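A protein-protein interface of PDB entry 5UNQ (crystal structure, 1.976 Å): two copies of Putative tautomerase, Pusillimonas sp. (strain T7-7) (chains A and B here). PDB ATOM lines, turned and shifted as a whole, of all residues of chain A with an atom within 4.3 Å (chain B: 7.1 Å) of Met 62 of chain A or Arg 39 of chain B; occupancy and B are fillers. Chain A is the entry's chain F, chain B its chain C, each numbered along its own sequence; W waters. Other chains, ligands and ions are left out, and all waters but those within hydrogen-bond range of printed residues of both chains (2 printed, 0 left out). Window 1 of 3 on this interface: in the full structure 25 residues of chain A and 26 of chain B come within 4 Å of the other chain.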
ATOM      1  N   THR A   4      -8.983 -15.787  21.374  1.00  0.00           N
ATOM      2  CA  THR A   4      -8.132 -16.694  20.616  1.00  0.00           C
ATOM      3  C   THR A   4      -8.918 -17.932  20.207  1.00  0.00           C
ATOM      4  O   THR A   4      -9.402 -18.685  21.053  1.00  0.00           O
ATOM      5  CB  THR A   4      -6.889 -17.111  21.420  1.00  0.00           C
ATOM      6  OG1 THR A   4      -6.156 -15.942  21.807  1.00  0.00           O
ATOM      7  CG2 THR A   4      -5.992 -18.008  20.582  1.00  0.00           C
ATOM      8  N   ILE A   5      -9.036 -18.137  18.899  1.00  0.00           N
ATOM      9  CA  ILE A   5      -9.878 -19.200  18.369  1.00  0.00           C
ATOM     10  C   ILE A   5      -9.064 -20.337  17.760  1.00  0.00           C
ATOM     11  O   ILE A   5      -8.191 -20.116  16.920  1.00  0.00           O
ATOM     12  CB  ILE A   5     -10.847 -18.655  17.306  1.00  0.00           C
ATOM     13  CG1 ILE A   5     -11.639 -17.473  17.870  1.00  0.00           C
ATOM     14  CG2 ILE A   5     -11.782 -19.750  16.821  1.00  0.00           C
ATOM     15  CD1 ILE A   5     -12.552 -16.812  16.859  1.00  0.00           C
ATOM     16  N   SER A   6      -9.359 -21.556  18.199  1.00  0.00           N
ATOM     17  CA  SER A   6      -8.736 -22.746  17.638  1.00  0.00           C
ATOM     18  C   SER A   6      -9.745 -23.500  16.785  1.00  0.00           C
ATOM     19  O   SER A   6     -10.761 -23.983  17.288  1.00  0.00           O
ATOM     20  CB  SER A   6      -8.190 -23.648  18.746  1.00  0.00           C
ATOM     21  OG  SER A   6      -7.156 -23.001  19.466  1.00  0.00           O
ATOM     22  N   TYR A  50      -5.847 -32.746  16.047  1.00  0.00           N
ATOM     23  CA  TYR A  50      -6.947 -32.570  16.987  1.00  0.00           C
ATOM     24  C   TYR A  50      -7.601 -33.903  17.322  1.00  0.00           C
ATOM     25  O   TYR A  50      -8.279 -34.502  16.488  1.00  0.00           O
ATOM     26  CB  TYR A  50      -7.984 -31.597  16.419  1.00  0.00           C
ATOM     27  CG  TYR A  50      -9.247 -31.476  17.245  1.00  0.00           C
ATOM     28  CD1 TYR A  50      -9.190 -31.231  18.613  1.00  0.00           C
ATOM     29  CD2 TYR A  50     -10.500 -31.590  16.653  1.00  0.00           C
ATOM     30  CE1 TYR A  50     -10.344 -31.115  19.368  1.00  0.00           C
ATOM     31  CE2 TYR A  50     -11.659 -31.472  17.397  1.00  0.00           C
ATOM     32  CZ  TYR A  50     -11.575 -31.236  18.754  1.00  0.00           C
ATOM     33  OH  TYR A  50     -12.729 -31.122  19.496  1.00  0.00           O
ATOM     34  N   LEU A  51      -7.384 -34.365  18.549  1.00  0.00           N
ATOM     35  CA  LEU A  51      -7.994 -35.604  19.014  1.00  0.00           C
ATOM     36  C   LEU A  51      -9.214 -35.297  19.873  1.00  0.00           C
ATOM     37  O   LEU A  51      -9.102 -34.702  20.946  1.00  0.00           O
ATOM     38  CB  LEU A  51      -6.987 -36.446  19.798  1.00  0.00           C
ATOM     39  CG  LEU A  51      -7.465 -37.851  20.173  1.00  0.00           C
ATOM     40  CD1 LEU A  51      -7.786 -38.653  18.922  1.00  0.00           C
ATOM     41  CD2 LEU A  51      -6.429 -38.568  21.021  1.00  0.00           C
ATOM     42  N   ASN A  52     -10.381 -35.705  19.387  1.00  0.00           N
ATOM     43  CA  ASN A  52     -11.641 -35.429  20.063  1.00  0.00           C
ATOM     44  C   ASN A  52     -12.317 -36.713  20.535  1.00  0.00           C
ATOM     45  O   ASN A  52     -12.876 -37.461  19.730  1.00  0.00           O
ATOM     46  CB  ASN A  52     -12.570 -34.645  19.132  1.00  0.00           C
ATOM     47  CG  ASN A  52     -13.946 -34.414  19.726  1.00  0.00           C
ATOM     48  OD1 ASN A  52     -14.131 -34.455  20.941  1.00  0.00           O
ATOM     49  ND2 ASN A  52     -14.924 -34.164  18.862  1.00  0.00           N
ATOM     50  N   LEU A  61     -13.909 -26.426  16.999  1.00  0.00           N
ATOM     51  CA  LEU A  61     -13.963 -24.976  17.142  1.00  0.00           C
ATOM     52  C   LEU A  61     -14.027 -24.596  18.615  1.00  0.00           C
ATOM     53  O   LEU A  61     -15.045 -24.803  19.276  1.00  0.00           O
ATOM     54  CB  LEU A  61     -15.165 -24.400  16.391  1.00  0.00           C
ATOM     55  CG  LEU A  61     -15.241 -22.874  16.316  1.00  0.00           C
ATOM     56  CD1 LEU A  61     -14.090 -22.324  15.494  1.00  0.00           C
ATOM     57  CD2 LEU A  61     -16.574 -22.433  15.739  1.00  0.00           C
ATOM     58  N   MET A  62     -12.933 -24.044  19.128  1.00  0.00           N
ATOM     59  CA  MET A  62     -12.836 -23.712  20.545  1.00  0.00           C
ATOM     60  C   MET A  62     -12.449 -22.252  20.762  1.00  0.00           C
ATOM     61  O   MET A  62     -11.506 -21.752  20.147  1.00  0.00           O
ATOM     62  CB  MET A  62     -11.826 -24.637  21.229  1.00  0.00           C
ATOM     63  CG  MET A  62     -12.317 -26.070  21.390  1.00  0.00           C
ATOM     64  SD  MET A  62     -10.986 -27.287  21.424  1.00  0.00           S
ATOM     65  CE  MET A  62     -10.508 -27.319  19.698  1.00  0.00           C
ATOM     66  N   PHE A  63     -13.187 -21.573  21.636  1.00  0.00           N
ATOM     67  CA  PHE A  63     -12.927 -20.170  21.949  1.00  0.00           C
ATOM     68  C   PHE A  63     -12.258 -20.010  23.310  1.00  0.00           C
ATOM     69  O   PHE A  63     -12.691 -20.607  24.297  1.00  0.00           O
ATOM     70  CB  PHE A  63     -14.227 -19.357  21.937  1.00  0.00           C
ATOM     71  CG  PHE A  63     -14.908 -19.299  20.598  1.00  0.00           C
ATOM     72  CD1 PHE A  63     -14.691 -18.231  19.744  1.00  0.00           C
ATOM     73  CD2 PHE A  63     -15.781 -20.299  20.206  1.00  0.00           C
ATOM     74  CE1 PHE A  63     -15.324 -18.168  18.518  1.00  0.00           C
ATOM     75  CE2 PHE A  63     -16.416 -20.242  18.978  1.00  0.00           C
ATOM     76  CZ  PHE A  63     -16.186 -19.174  18.133  1.00  0.00           C
ATOM     77  N   VAL A  64     -11.207 -19.199  23.359  1.00  0.00           N
ATOM     78  CA  VAL A  64     -10.584 -18.829  24.626  1.00  0.00           C
ATOM     79  C   VAL A  64     -10.512 -17.312  24.748  1.00  0.00           C
ATOM     80  O   VAL A  64      -9.913 -16.645  23.904  1.00  0.00           O
ATOM     81  CB  VAL A  64      -9.166 -19.413  24.769  1.00  0.00           C
ATOM     82  CG1 VAL A  64      -8.608 -19.105  26.150  1.00  0.00           C
ATOM     83  CG2 VAL A  64      -9.181 -20.911  24.522  1.00  0.00           C
ATOM     84  N   GLU A  97     -20.602 -29.291  20.137  1.00  0.00           N
ATOM     85  CA  GLU A  97     -19.172 -29.485  19.935  1.00  0.00           C
ATOM     86  C   GLU A  97     -18.377 -28.211  20.217  1.00  0.00           C
ATOM     87  O   GLU A  97     -17.258 -28.272  20.728  1.00  0.00           O
ATOM     88  CB  GLU A  97     -18.898 -29.968  18.509  1.00  0.00           C
ATOM     89  CG  GLU A  97     -19.413 -31.371  18.225  1.00  0.00           C
ATOM     90  CD  GLU A  97     -18.730 -32.424  19.074  1.00  0.00           C
ATOM     91  OE1 GLU A  97     -17.509 -32.300  19.308  1.00  0.00           O
ATOM     92  OE2 GLU A  97     -19.414 -33.375  19.507  1.00  0.00           O
ATOM     93  N   ARG A  99     -16.883 -25.056  21.950  1.00  0.00           N
ATOM     94  CA  ARG A  99     -16.542 -24.759  23.339  1.00  0.00           C
ATOM     95  C   ARG A  99     -16.020 -23.331  23.508  1.00  0.00           C
ATOM     96  O   ARG A  99     -15.404 -22.776  22.599  1.00  0.00           O
ATOM     97  CB  ARG A  99     -15.501 -25.754  23.856  1.00  0.00           C
ATOM     98  CG  ARG A  99     -15.993 -27.188  23.956  1.00  0.00           C
ATOM     99  CD  ARG A  99     -17.038 -27.340  25.051  1.00  0.00           C
ATOM    100  NE  ARG A  99     -17.335 -28.741  25.334  1.00  0.00           N
ATOM    101  CZ  ARG A  99     -18.204 -29.475  24.647  1.00  0.00           C
ATOM    102  NH1 ARG A  99     -18.410 -30.743  24.977  1.00  0.00           N
ATOM    103  NH2 ARG A  99     -18.866 -28.943  23.629  1.00  0.00           N
ATOM    104  N   PRO B   1     -11.603 -31.570  29.744  1.00  0.00           N
ATOM    105  CA  PRO B   1     -10.180 -31.234  29.861  1.00  0.00           C
ATOM    106  C   PRO B   1      -9.528 -31.005  28.502  1.00  0.00           C
ATOM    107  O   PRO B   1      -9.707 -31.812  27.590  1.00  0.00           O
ATOM    108  CB  PRO B   1      -9.584 -32.465  30.550  1.00  0.00           C
ATOM    109  CG  PRO B   1     -10.723 -33.061  31.299  1.00  0.00           C
ATOM    110  CD  PRO B   1     -11.936 -32.817  30.452  1.00  0.00           C
ATOM    111  N   TYR B   2      -8.779 -29.915  28.375  1.00  0.00           N
ATOM    112  CA  TYR B   2      -8.113 -29.583  27.121  1.00  0.00           C
ATOM    113  C   TYR B   2      -6.602 -29.710  27.265  1.00  0.00           C
ATOM    114  O   TYR B   2      -5.995 -29.039  28.096  1.00  0.00           O
ATOM    115  CB  TYR B   2      -8.477 -28.164  26.673  1.00  0.00           C
ATOM    116  CG  TYR B   2      -9.964 -27.894  26.620  1.00  0.00           C
ATOM    117  CD1 TYR B   2     -10.665 -27.526  27.762  1.00  0.00           C
ATOM    118  CD2 TYR B   2     -10.668 -28.001  25.427  1.00  0.00           C
ATOM    119  CE1 TYR B   2     -12.021 -27.280  27.721  1.00  0.00           C
ATOM    120  CE2 TYR B   2     -12.027 -27.755  25.376  1.00  0.00           C
ATOM    121  CZ  TYR B   2     -12.698 -27.394  26.526  1.00  0.00           C
ATOM    122  OH  TYR B   2     -14.050 -27.146  26.487  1.00  0.00           O
ATOM    123  N   VAL B   3      -5.998 -30.574  26.456  1.00  0.00           N
ATOM    124  CA  VAL B   3      -4.547 -30.718  26.448  1.00  0.00           C
ATOM    125  C   VAL B   3      -3.956 -30.103  25.187  1.00  0.00           C
ATOM    126  O   VAL B   3      -4.134 -30.626  24.086  1.00  0.00           O
ATOM    127  CB  VAL B   3      -4.121 -32.192  26.542  1.00  0.00           C
ATOM    128  CG1 VAL B   3      -2.603 -32.301  26.567  1.00  0.00           C
ATOM    129  CG2 VAL B   3      -4.722 -32.836  27.778  1.00  0.00           C
ATOM    130  N   THR B   4      -3.254 -28.987  25.349  1.00  0.00           N
ATOM    131  CA  THR B   4      -2.640 -28.309  24.214  1.00  0.00           C
ATOM    132  C   THR B   4      -1.133 -28.533  24.208  1.00  0.00           C
ATOM    133  O   THR B   4      -0.427 -28.128  25.132  1.00  0.00           O
ATOM    134  CB  THR B   4      -2.938 -26.802  24.226  1.00  0.00           C
ATOM    135  OG1 THR B   4      -4.356 -26.598  24.275  1.00  0.00           O
ATOM    136  CG2 THR B   4      -2.378 -26.140  22.976  1.00  0.00           C
ATOM    137  N   SER B  24      -4.213 -38.663  25.472  1.00  0.00           N
ATOM    138  CA  SER B  24      -5.606 -38.868  25.844  1.00  0.00           C
ATOM    139  C   SER B  24      -5.715 -39.929  26.936  1.00  0.00           C
ATOM    140  O   SER B  24      -6.465 -39.765  27.899  1.00  0.00           O
ATOM    141  CB  SER B  24      -6.435 -39.273  24.624  1.00  0.00           C
ATOM    142  OG  SER B  24      -7.811 -39.378  24.951  1.00  0.00           O
ATOM    143  N   VAL B  27      -4.675 -38.664  30.395  1.00  0.00           N
ATOM    144  CA  VAL B  27      -5.696 -37.872  31.070  1.00  0.00           C
ATOM    145  C   VAL B  27      -6.747 -38.767  31.719  1.00  0.00           C
ATOM    146  O   VAL B  27      -7.083 -38.597  32.892  1.00  0.00           O
ATOM    147  CB  VAL B  27      -6.389 -36.899  30.101  1.00  0.00           C
ATOM    148  CG1 VAL B  27      -7.520 -36.161  30.803  1.00  0.00           C
ATOM    149  CG2 VAL B  27      -5.379 -35.918  29.529  1.00  0.00           C
ATOM    150  N   PRO B  34     -13.756 -38.926  31.863  1.00  0.00           N
ATOM    151  CA  PRO B  34     -14.399 -39.694  30.793  1.00  0.00           C
ATOM    152  C   PRO B  34     -13.752 -39.394  29.445  1.00  0.00           C
ATOM    153  O   PRO B  34     -13.456 -38.233  29.161  1.00  0.00           O
ATOM    154  CB  PRO B  34     -15.851 -39.207  30.827  1.00  0.00           C
ATOM    155  CG  PRO B  34     -16.037 -38.649  32.201  1.00  0.00           C
ATOM    156  CD  PRO B  34     -14.712 -38.059  32.573  1.00  0.00           C
ATOM    157  N   LEU B  35     -13.531 -40.428  28.640  1.00  0.00           N
ATOM    158  CA  LEU B  35     -12.898 -40.276  27.333  1.00  0.00           C
ATOM    159  C   LEU B  35     -13.666 -39.301  26.444  1.00  0.00           C
ATOM    160  O   LEU B  35     -13.074 -38.565  25.654  1.00  0.00           O
ATOM    161  CB  LEU B  35     -12.776 -41.637  26.641  1.00  0.00           C
ATOM    162  CG  LEU B  35     -12.286 -41.666  25.191  1.00  0.00           C
ATOM    163  CD1 LEU B  35     -10.918 -41.008  25.056  1.00  0.00           C
ATOM    164  CD2 LEU B  35     -12.250 -43.097  24.669  1.00  0.00           C
ATOM    165  N   ALA B  36     -14.987 -39.287  26.595  1.00  0.00           N
ATOM    166  CA  ALA B  36     -15.854 -38.450  25.771  1.00  0.00           C
ATOM    167  C   ALA B  36     -15.622 -36.953  25.992  1.00  0.00           C
ATOM    168  O   ALA B  36     -16.063 -36.130  25.191  1.00  0.00           O
ATOM    169  CB  ALA B  36     -17.312 -38.797  26.035  1.00  0.00           C
ATOM    170  N   SER B  37     -14.929 -36.603  27.071  1.00  0.00           N
ATOM    171  CA  SER B  37     -14.712 -35.201  27.411  1.00  0.00           C
ATOM    172  C   SER B  37     -13.265 -34.759  27.202  1.00  0.00           C
ATOM    173  O   SER B  37     -12.935 -33.590  27.402  1.00  0.00           O
ATOM    174  CB  SER B  37     -15.119 -34.941  28.864  1.00  0.00           C
ATOM    175  OG  SER B  37     -14.218 -35.567  29.763  1.00  0.00           O
ATOM    176  N   VAL B  38     -12.405 -35.690  26.802  1.00  0.00           N
ATOM    177  CA  VAL B  38     -10.983 -35.396  26.666  1.00  0.00           C
ATOM    178  C   VAL B  38     -10.619 -34.932  25.257  1.00  0.00           C
ATOM    179  O   VAL B  38     -10.933 -35.600  24.271  1.00  0.00           O
ATOM    180  CB  VAL B  38     -10.121 -36.621  27.028  1.00  0.00           C
ATOM    181  CG1 VAL B  38      -8.643 -36.298  26.875  1.00  0.00           C
ATOM    182  CG2 VAL B  38     -10.429 -37.081  28.448  1.00  0.00           C
ATOM    183  N   ARG B  39      -9.959 -33.780  25.173  1.00  0.00           N
ATOM    184  CA  ARG B  39      -9.518 -33.229  23.896  1.00  0.00           C
ATOM    185  C   ARG B  39      -8.018 -32.952  23.902  1.00  0.00           C
ATOM    186  O   ARG B  39      -7.468 -32.490  24.903  1.00  0.00           O
ATOM    187  CB  ARG B  39     -10.282 -31.944  23.571  1.00  0.00           C
ATOM    188  CG  ARG B  39     -11.783 -32.125  23.462  1.00  0.00           C
ATOM    189  CD  ARG B  39     -12.458 -30.841  23.021  1.00  0.00           C
ATOM    190  NE  ARG B  39     -13.878 -31.037  22.755  1.00  0.00           N
ATOM    191  CZ  ARG B  39     -14.657 -30.141  22.160  1.00  0.00           C
ATOM    192  NH1 ARG B  39     -14.150 -28.982  21.762  1.00  0.00           N
ATOM    193  NH2 ARG B  39     -15.940 -30.404  21.956  1.00  0.00           N
ATOM    194  N   VAL B  40      -7.360 -33.237  22.783  1.00  0.00           N
ATOM    195  CA  VAL B  40      -5.932 -32.965  22.649  1.00  0.00           C
ATOM    196  C   VAL B  40      -5.649 -32.174  21.376  1.00  0.00           C
ATOM    197  O   VAL B  40      -6.029 -32.588  20.282  1.00  0.00           O
ATOM    198  CB  VAL B  40      -5.095 -34.262  22.629  1.00  0.00           C
ATOM    199  CG1 VAL B  40      -3.615 -33.931  22.713  1.00  0.00           C
ATOM    200  CG2 VAL B  40      -5.496 -35.182  23.774  1.00  0.00           C
ATOM    201  N   MET B  41      -4.986 -31.032  21.526  1.00  0.00           N
ATOM    202  CA  MET B  41      -4.623 -30.198  20.385  1.00  0.00           C
ATOM    203  C   MET B  41      -3.107 -30.104  20.248  1.00  0.00           C
ATOM    204  O   MET B  41      -2.385 -30.081  21.244  1.00  0.00           O
ATOM    205  CB  MET B  41      -5.228 -28.797  20.522  1.00  0.00           C
ATOM    206  CG  MET B  41      -6.727 -28.729  20.266  1.00  0.00           C
ATOM    207  SD  MET B  41      -7.729 -29.482  21.564  1.00  0.00           S
ATOM    208  CE  MET B  41      -7.371 -28.394  22.942  1.00  0.00           C
ATOM    209  N   ALA B 113     -20.964 -27.975  26.528  1.00  0.00           N
ATOM    210  CA  ALA B 113     -21.813 -28.173  25.360  1.00  0.00           C
ATOM    211  C   ALA B 113     -23.089 -27.347  25.480  1.00  0.00           C
ATOM    212  O   ALA B 113     -23.692 -27.274  26.551  1.00  0.00           O
ATOM    213  CB  ALA B 113     -22.147 -29.648  25.184  1.00  0.00           C
HETATM  214  O   HOH W   1     -14.860 -28.126  18.924  1.00  0.00           O
HETATM  215  O   HOH W   2     -16.579 -33.012  22.178  1.00  0.00           O
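The backbone carbonyl oxygen (O) of Ser 6 of chain A sits at hydrogen-bond distance from the backbone NH (N) of Met 62 of chain A (2.8 Å).
The side-chain carboxylate (OE1) of Glu 97 of chain A is in hydrogen-bond range of the side-chain amide nitrogen (ND2) of Asn 52 of chain A.
The backbone NH (N) of Phe 63 of chain A sits at hydrogen-bond distance from the backbone carbonyl oxygen (O) of Arg 99 of chain A, at 2.7 Å.
The guanidinium group (NH2) of Arg 99 of chain A sits at hydrogen-bond distance from the backbone carbonyl oxygen (O) of Glu 97 of chain A (3.4 Å).
The backbone NH of Arg 39 of chain B is in hydrogen-bond range of the backbone carbonyl oxygen of Pro 1 of chain B, 3.1 Å away.
The backbone carbonyl oxygen (O) of Val 3 of chain B is in hydrogen-bond range of the backbone NH (N) of Met 41 of chain B (2.7 Å).
Position printed for both chains: 4.
Water W2 lies within hydrogen-bond range of NH2 of Arg 39 of chain B (2.7 Å), OE1 of Glu 97 of chain A (3.1 Å) and OD1 of Asn 52 of chain A (3.1 Å).
Water W1 lies within hydrogen-bond range of the backbone NH (N) of Leu 61 of chain A (2.7 Å), the backbone carbonyl oxygen (O) of Glu 97 of chain A (3.0 Å) and the guanidinium group (NH1) of Arg 39 of chain B (3.0 Å).
Among the printed residues, pairs that only touch across the chains: Arg 99 of chain A with Tyr 2 of chain B, Leu 51 of chain A with Arg 39 of chain B, Arg 99 of chain A with Arg 39 of chain B, Tyr 50 of chain A with Val 40 of chain B, Arg 99 of chain A with Ala 113 of chain B, Leu 51 of chain A with Ser 24 of chain B, Tyr 50 of chain A with Met 41 of chain B, Asn 52 of chain A with Arg 39 of chain B, Leu 51 of chain A with Val 38 of chain B and Met 62 of chain A with Met 41 of chain B.
Of the 12 printed residues of chain A, 6 touch a printed residue of chain B.
Printed residues of chain A that touch a printed residue of chain B: Tyr 50, Leu 51, Asn 52, Met 62, Glu 97 and Arg 99.
Among the printed residues, 14 pairs touch across the chains.
Among the printed residues, Asp or Glu carboxylates within 4 Å of a Lys or Arg side-chain nitrogen of the other chain: Glu 97 of chain A with Arg 39 of chain B.
OH of Tyr 50 of chain A is in hydrogen-bond range of NH1 of Arg 39 of chain B (3.4 Å).
The backbone carbonyl oxygen of Val 40 of chain B is in hydrogen-bond range of the backbone NH of Leu 51 of chain A, 2.8 Å away.
The guanidinium group of Arg 39 of chain B sits close to the side-chain sulfur of Met 62 of chain A, at 3.6 Å.
The guanidinium group of Arg 39 of chain B is in salt-bridge range of the side-chain carboxylate of Glu 97 of chain A (3.6 Å).
Met 62 of chain A touches just these residues of chain B: Arg 39 (3.5 Å) and Met 41 (3.9 Å).
Of chain A, only Tyr 50, Leu 51, Asn 52, Met 62, Glu 97 and Arg 99 come within 4 Å of Arg 39 of chain B.
Of the printed residues of chain B, Arg 99 of chain A touches Tyr 2 (3.2 Å), Arg 39 (3.4 Å) and Ala 113 (3.5 Å).
Of the printed residues of chain A, Met 41 of chain B touches Tyr 50 (3.7 Å) and Met 62 (3.9 Å).
Of the printed residues of chain B, Leu 51 of chain A touches Ser 24, Val 38, Arg 39 and Val 40.
The nearest residue of chain B that does not touch Met 62 of chain A is Tyr 2 of chain B (4.1 Å).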
